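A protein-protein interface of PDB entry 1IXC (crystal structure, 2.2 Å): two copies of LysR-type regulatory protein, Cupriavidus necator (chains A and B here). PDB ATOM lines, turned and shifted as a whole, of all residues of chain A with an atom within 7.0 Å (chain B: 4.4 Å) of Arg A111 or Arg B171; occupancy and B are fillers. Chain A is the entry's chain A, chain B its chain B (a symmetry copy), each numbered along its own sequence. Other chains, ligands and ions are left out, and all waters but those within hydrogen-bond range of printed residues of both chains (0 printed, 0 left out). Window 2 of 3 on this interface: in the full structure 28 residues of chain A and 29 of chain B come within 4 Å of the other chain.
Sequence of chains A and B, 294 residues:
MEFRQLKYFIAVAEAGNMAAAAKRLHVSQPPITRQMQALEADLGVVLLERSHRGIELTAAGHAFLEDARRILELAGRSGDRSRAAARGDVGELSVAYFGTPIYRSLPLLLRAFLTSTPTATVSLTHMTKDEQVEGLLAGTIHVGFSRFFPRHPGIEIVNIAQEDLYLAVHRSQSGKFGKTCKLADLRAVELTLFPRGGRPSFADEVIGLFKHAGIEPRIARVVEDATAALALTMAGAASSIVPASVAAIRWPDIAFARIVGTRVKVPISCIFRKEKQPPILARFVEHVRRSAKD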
ATOM      1  N   ARG A 104     -11.684  13.788   1.152  1.00  0.00           N
ATOM      2  CA  ARG A 104     -11.242  15.001   1.824  1.00  0.00           C
ATOM      3  C   ARG A 104      -9.823  14.933   2.361  1.00  0.00           C
ATOM      4  O   ARG A 104      -8.962  15.758   2.016  1.00  0.00           O
ATOM      5  CB  ARG A 104     -12.189  15.305   2.990  1.00  0.00           C
ATOM      6  CG  ARG A 104     -11.956  16.642   3.653  1.00  0.00           C
ATOM      7  CD  ARG A 104     -12.101  17.832   2.706  1.00  0.00           C
ATOM      8  NE  ARG A 104     -11.953  19.105   3.418  1.00  0.00           N
ATOM      9  CZ  ARG A 104     -11.494  20.223   2.880  1.00  0.00           C
ATOM     10  NH1 ARG A 104     -11.141  20.260   1.608  1.00  0.00           N
ATOM     11  NH2 ARG A 104     -11.401  21.323   3.619  1.00  0.00           N
ATOM     12  N   LEU A 106      -7.291  13.016   1.818  1.00  0.00           N
ATOM     13  CA  LEU A 106      -6.195  12.846   0.868  1.00  0.00           C
ATOM     14  C   LEU A 106      -5.930  14.109   0.047  1.00  0.00           C
ATOM     15  O   LEU A 106      -4.783  14.503  -0.107  1.00  0.00           O
ATOM     16  CB  LEU A 106      -6.372  11.588   0.012  1.00  0.00           C
ATOM     17  CG  LEU A 106      -5.373  11.363  -1.120  1.00  0.00           C
ATOM     18  CD1 LEU A 106      -3.911  11.470  -0.645  1.00  0.00           C
ATOM     19  CD2 LEU A 106      -5.609   9.998  -1.745  1.00  0.00           C
ATOM     20  N   PRO A 107      -6.955  14.724  -0.531  1.00  0.00           N
ATOM     21  CA  PRO A 107      -6.788  16.022  -1.190  1.00  0.00           C
ATOM     22  C   PRO A 107      -6.093  17.088  -0.346  1.00  0.00           C
ATOM     23  O   PRO A 107      -5.207  17.786  -0.866  1.00  0.00           O
ATOM     24  CB  PRO A 107      -8.225  16.433  -1.506  1.00  0.00           C
ATOM     25  CG  PRO A 107      -8.931  15.112  -1.750  1.00  0.00           C
ATOM     26  CD  PRO A 107      -8.293  14.159  -0.770  1.00  0.00           C
ATOM     27  N   LEU A 108      -6.462  17.205   0.923  1.00  0.00           N
ATOM     28  CA  LEU A 108      -5.840  18.169   1.825  1.00  0.00           C
ATOM     29  C   LEU A 108      -4.330  17.919   2.013  1.00  0.00           C
ATOM     30  O   LEU A 108      -3.534  18.843   2.015  1.00  0.00           O
ATOM     31  CB  LEU A 108      -6.539  18.127   3.180  1.00  0.00           C
ATOM     32  CG  LEU A 108      -7.848  18.918   3.312  1.00  0.00           C
ATOM     33  CD1 LEU A 108      -8.318  18.822   4.777  1.00  0.00           C
ATOM     34  CD2 LEU A 108      -7.703  20.383   2.901  1.00  0.00           C
ATOM     35  N   LEU A 109      -3.946  16.659   2.177  1.00  0.00           N
ATOM     36  CA  LEU A 109      -2.530  16.299   2.319  1.00  0.00           C
ATOM     37  C   LEU A 109      -1.796  16.555   0.984  1.00  0.00           C
ATOM     38  O   LEU A 109      -0.698  17.128   0.964  1.00  0.00           O
ATOM     39  CB  LEU A 109      -2.438  14.843   2.765  1.00  0.00           C
ATOM     40  CG  LEU A 109      -1.121  14.085   2.876  1.00  0.00           C
ATOM     41  CD1 LEU A 109      -1.477  12.682   3.320  1.00  0.00           C
ATOM     42  CD2 LEU A 109      -0.345  14.008   1.594  1.00  0.00           C
ATOM     43  N   LEU A 110      -2.414  16.180  -0.136  1.00  0.00           N
ATOM     44  CA  LEU A 110      -1.820  16.497  -1.445  1.00  0.00           C
ATOM     45  C   LEU A 110      -1.635  18.007  -1.672  1.00  0.00           C
ATOM     46  O   LEU A 110      -0.643  18.422  -2.268  1.00  0.00           O
ATOM     47  CB  LEU A 110      -2.615  15.882  -2.582  1.00  0.00           C
ATOM     48  CG  LEU A 110      -2.611  14.342  -2.597  1.00  0.00           C
ATOM     49  CD1 LEU A 110      -3.617  13.818  -3.606  1.00  0.00           C
ATOM     50  CD2 LEU A 110      -1.222  13.793  -2.894  1.00  0.00           C
ATOM     51  N   ARG A 111      -2.574  18.824  -1.190  1.00  0.00           N
ATOM     52  CA  ARG A 111      -2.474  20.260  -1.357  1.00  0.00           C
ATOM     53  C   ARG A 111      -1.238  20.819  -0.635  1.00  0.00           C
ATOM     54  O   ARG A 111      -0.470  21.593  -1.202  1.00  0.00           O
ATOM     55  CB  ARG A 111      -3.714  20.978  -0.829  1.00  0.00           C
ATOM     56  CG  ARG A 111      -3.723  22.456  -1.236  1.00  0.00           C
ATOM     57  CD  ARG A 111      -4.642  23.349  -0.461  1.00  0.00           C
ATOM     58  NE  ARG A 111      -4.752  24.651  -1.131  1.00  0.00           N
ATOM     59  CZ  ARG A 111      -4.781  25.830  -0.518  1.00  0.00           C
ATOM     60  NH1 ARG A 111      -4.697  25.915   0.810  1.00  0.00           N
ATOM     61  NH2 ARG A 111      -4.886  26.945  -1.240  1.00  0.00           N
ATOM     62  N   ALA A 112      -1.081  20.440   0.626  1.00  0.00           N
ATOM     63  CA  ALA A 112       0.074  20.848   1.418  1.00  0.00           C
ATOM     64  C   ALA A 112       1.376  20.410   0.747  1.00  0.00           C
ATOM     65  O   ALA A 112       2.362  21.135   0.766  1.00  0.00           O
ATOM     66  CB  ALA A 112      -0.028  20.277   2.822  1.00  0.00           C
ATOM     67  N   PHE A 113       1.382  19.233   0.134  1.00  0.00           N
ATOM     68  CA  PHE A 113       2.593  18.754  -0.540  1.00  0.00           C
ATOM     69  C   PHE A 113       2.888  19.609  -1.752  1.00  0.00           C
ATOM     70  O   PHE A 113       4.027  19.999  -1.960  1.00  0.00           O
ATOM     71  CB  PHE A 113       2.453  17.303  -0.974  1.00  0.00           C
ATOM     72  CG  PHE A 113       3.547  16.827  -1.890  1.00  0.00           C
ATOM     73  CD1 PHE A 113       4.848  16.656  -1.418  1.00  0.00           C
ATOM     74  CD2 PHE A 113       3.275  16.518  -3.216  1.00  0.00           C
ATOM     75  CE1 PHE A 113       5.849  16.195  -2.265  1.00  0.00           C
ATOM     76  CE2 PHE A 113       4.274  16.050  -4.064  1.00  0.00           C
ATOM     77  CZ  PHE A 113       5.557  15.891  -3.594  1.00  0.00           C
ATOM     78  N   LEU A 114       1.859  19.914  -2.540  1.00  0.00           N
ATOM     79  CA  LEU A 114       2.034  20.713  -3.753  1.00  0.00           C
ATOM     80  C   LEU A 114       2.406  22.161  -3.433  1.00  0.00           C
ATOM     81  O   LEU A 114       3.126  22.792  -4.195  1.00  0.00           O
ATOM     82  CB  LEU A 114       0.782  20.667  -4.646  1.00  0.00           C
ATOM     83  CG  LEU A 114       0.461  19.296  -5.253  1.00  0.00           C
ATOM     84  CD1 LEU A 114      -0.904  19.309  -5.934  1.00  0.00           C
ATOM     85  CD2 LEU A 114       1.525  18.871  -6.231  1.00  0.00           C
ATOM     86  N   THR A 115       1.928  22.682  -2.307  1.00  0.00           N
ATOM     87  CA  THR A 115       2.267  24.051  -1.901  1.00  0.00           C
ATOM     88  C   THR A 115       3.746  24.180  -1.611  1.00  0.00           C
ATOM     89  O   THR A 115       4.382  25.129  -2.041  1.00  0.00           O
ATOM     90  CB  THR A 115       1.496  24.460  -0.642  1.00  0.00           C
ATOM     91  OG1 THR A 115       0.090  24.408  -0.890  1.00  0.00           O
ATOM     92  CG2 THR A 115       1.762  25.922  -0.303  1.00  0.00           C
ATOM     93  N   SER A 116       4.286  23.230  -0.858  1.00  0.00           N
ATOM     94  CA  SER A 116       5.702  23.230  -0.542  1.00  0.00           C
ATOM     95  C   SER A 116       6.571  22.759  -1.713  1.00  0.00           C
ATOM     96  O   SER A 116       7.767  22.970  -1.698  1.00  0.00           O
ATOM     97  CB  SER A 116       5.953  22.348   0.676  1.00  0.00           C
ATOM     98  OG  SER A 116       5.832  20.991   0.322  1.00  0.00           O
ATOM     99  N   THR A 117       5.971  22.148  -2.734  1.00  0.00           N
ATOM    100  CA  THR A 117       6.720  21.570  -3.859  1.00  0.00           C
ATOM    101  C   THR A 117       6.135  22.023  -5.209  1.00  0.00           C
ATOM    102  O   THR A 117       5.601  21.222  -5.966  1.00  0.00           O
ATOM    103  CB  THR A 117       6.652  20.043  -3.736  1.00  0.00           C
ATOM    104  OG1 THR A 117       6.886  19.660  -2.370  1.00  0.00           O
ATOM    105  CG2 THR A 117       7.751  19.365  -4.526  1.00  0.00           C
ATOM    106  N   HIS A 287       7.425  14.701   3.688  1.00  0.00           N
ATOM    107  CA  HIS A 287       6.172  15.425   3.940  1.00  0.00           C
ATOM    108  C   HIS A 287       5.142  14.603   4.728  1.00  0.00           C
ATOM    109  O   HIS A 287       4.498  15.128   5.622  1.00  0.00           O
ATOM    110  CB  HIS A 287       5.542  15.895   2.624  1.00  0.00           C
ATOM    111  CG  HIS A 287       4.138  16.405   2.767  1.00  0.00           C
ATOM    112  ND1 HIS A 287       3.846  17.665   3.236  1.00  0.00           N
ATOM    113  CD2 HIS A 287       2.946  15.827   2.476  1.00  0.00           C
ATOM    114  CE1 HIS A 287       2.536  17.838   3.247  1.00  0.00           C
ATOM    115  NE2 HIS A 287       1.965  16.740   2.782  1.00  0.00           N
ATOM    116  N   VAL B 169     -13.511  25.084  -9.803  1.00  0.00           N
ATOM    117  CA  VAL B 169     -12.185  25.612  -9.488  1.00  0.00           C
ATOM    118  C   VAL B 169     -11.962  25.595  -7.983  1.00  0.00           C
ATOM    119  O   VAL B 169     -12.914  25.539  -7.213  1.00  0.00           O
ATOM    120  CB  VAL B 169     -12.022  27.068  -9.986  1.00  0.00           C
ATOM    121  CG1 VAL B 169     -12.021  27.127 -11.491  1.00  0.00           C
ATOM    122  CG2 VAL B 169     -13.133  27.968  -9.447  1.00  0.00           C
ATOM    123  N   HIS B 170     -10.707  25.637  -7.566  1.00  0.00           N
ATOM    124  CA  HIS B 170     -10.395  25.727  -6.159  1.00  0.00           C
ATOM    125  C   HIS B 170     -11.022  27.002  -5.595  1.00  0.00           C
ATOM    126  O   HIS B 170     -11.209  27.990  -6.314  1.00  0.00           O
ATOM    127  CB  HIS B 170      -8.881  25.725  -5.927  1.00  0.00           C
ATOM    128  CG  HIS B 170      -8.505  25.618  -4.483  1.00  0.00           C
ATOM    129  ND1 HIS B 170      -8.691  24.462  -3.754  1.00  0.00           N
ATOM    130  CD2 HIS B 170      -8.018  26.534  -3.614  1.00  0.00           C
ATOM    131  CE1 HIS B 170      -8.293  24.657  -2.509  1.00  0.00           C
ATOM    132  NE2 HIS B 170      -7.877  25.906  -2.397  1.00  0.00           N
ATOM    133  N   ARG B 171     -11.354  26.965  -4.313  1.00  0.00           N
ATOM    134  CA  ARG B 171     -11.987  28.083  -3.616  1.00  0.00           C
ATOM    135  C   ARG B 171     -11.286  29.430  -3.853  1.00  0.00           C
ATOM    136  O   ARG B 171     -11.936  30.468  -3.981  1.00  0.00           O
ATOM    137  CB  ARG B 171     -12.058  27.728  -2.110  1.00  0.00           C
ATOM    138  CG  ARG B 171     -11.530  28.746  -1.101  1.00  0.00           C
ATOM    139  CD  ARG B 171     -10.662  28.119   0.023  1.00  0.00           C
ATOM    140  NE  ARG B 171      -9.276  28.602  -0.024  1.00  0.00           N
ATOM    141  CZ  ARG B 171      -8.304  28.231   0.808  1.00  0.00           C
ATOM    142  NH1 ARG B 171      -8.532  27.339   1.772  1.00  0.00           N
ATOM    143  NH2 ARG B 171      -7.089  28.757   0.673  1.00  0.00           N
ATOM    144  N   SER B 172      -9.963  29.390  -3.965  1.00  0.00           N
ATOM    145  CA  SER B 172      -9.145  30.589  -4.061  1.00  0.00           C
ATOM    146  C   SER B 172      -9.180  31.241  -5.436  1.00  0.00           C
ATOM    147  O   SER B 172      -8.772  32.393  -5.587  1.00  0.00           O
ATOM    148  CB  SER B 172      -7.705  30.252  -3.683  1.00  0.00           C
ATOM    149  OG  SER B 172      -7.075  29.504  -4.707  1.00  0.00           O
ATOM    150  N   GLN B 173      -9.638  30.501  -6.439  1.00  0.00           N
ATOM    151  CA  GLN B 173      -9.786  31.050  -7.779  1.00  0.00           C
ATOM    152  C   GLN B 173     -11.222  31.487  -8.026  1.00  0.00           C
ATOM    153  O   GLN B 173     -11.561  31.899  -9.134  1.00  0.00           O
ATOM    154  CB  GLN B 173      -9.372  30.034  -8.838  1.00  0.00           C
ATOM    155  CG  GLN B 173      -7.986  29.486  -8.666  1.00  0.00           C
ATOM    156  CD  GLN B 173      -6.946  30.569  -8.456  1.00  0.00           C
ATOM    157  OE1 GLN B 173      -6.672  31.361  -9.361  1.00  0.00           O
ATOM    158  NE2 GLN B 173      -6.356  30.602  -7.260  1.00  0.00           N
ATOM    159  N   SER B 174     -12.072  31.380  -7.006  1.00  0.00           N
ATOM    160  CA  SER B 174     -13.461  31.834  -7.113  1.00  0.00           C
ATOM    161  C   SER B 174     -13.499  33.359  -7.115  1.00  0.00           C
ATOM    162  O   SER B 174     -12.823  33.999  -6.308  1.00  0.00           O
ATOM    163  CB  SER B 174     -14.298  31.306  -5.948  1.00  0.00           C
ATOM    164  OG  SER B 174     -14.224  32.176  -4.828  1.00  0.00           O
ATOM    165  N   ALA B 235      -7.564  19.818  -4.231  1.00  0.00           N
ATOM    166  CA  ALA B 235      -6.149  19.922  -3.802  1.00  0.00           C
ATOM    167  C   ALA B 235      -5.447  21.172  -4.378  1.00  0.00           C
ATOM    168  O   ALA B 235      -4.257  21.365  -4.137  1.00  0.00           O
ATOM    169  CB  ALA B 235      -5.425  18.667  -4.222  1.00  0.00           C
ATOM    170  N   ASP B 253     -13.803  23.581  -0.438  1.00  0.00           N
ATOM    171  CA  ASP B 253     -12.736  24.150  -1.250  1.00  0.00           C
ATOM    172  C   ASP B 253     -12.963  24.149  -2.753  1.00  0.00           C
ATOM    173  O   ASP B 253     -12.112  24.629  -3.491  1.00  0.00           O
ATOM    174  CB  ASP B 253     -11.386  23.522  -0.917  1.00  0.00           C
ATOM    175  CG  ASP B 253     -11.011  23.713   0.526  1.00  0.00           C
ATOM    176  OD1 ASP B 253     -11.452  24.712   1.131  1.00  0.00           O
ATOM    177  OD2 ASP B 253     -10.294  22.910   1.143  1.00  0.00           O
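NH2 of Arg A111 sits close to NH2 of Arg B171 (3.4 Å).
NE2 of His B170 is in hydrogen-bond range of NH2 of Arg A111, at 3.4 Å.
OD2 of Asp B253 is in salt-bridge range of NH1 of Arg A104 (2.8 Å).
OG1 of Thr A115 lies within hydrogen-bond range of O of Arg A111.
A ring nitrogen (ND1) of His B170 sits close to the backbone carbonyl oxygen of Asp B253 (3.4 Å).
O of Arg B171 is in hydrogen-bond range of OG of Ser B174, at 3.0 Å.
The guanidinium group of Arg B171 is in salt-bridge range of the side-chain carboxylate of Asp B253.
Among the printed residues, merely in contact across the chains: Arg A111 with Ala B235 (3.1 Å) and Pro A107 with Ala B235 (3.5 Å).
Of the printed residues of chain B, Pro A107 touches Ala B235.
Of chain A, only Arg A111 (3.4 Å) comes within 4 Å of Arg B171.
Of the printed residues of chain A, Ala B235 touches Pro A107 and Arg A111.
Printed residues of chain A within 4 Å of Asp B253: Arg A104 (2.8 Å).
Printed residues of chain B that touch a printed residue of chain A: His B170, Arg B171, Ala B235 and Asp B253.
Among the printed residues, 5 pairs touch across the chains.
No position is printed for both chains.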
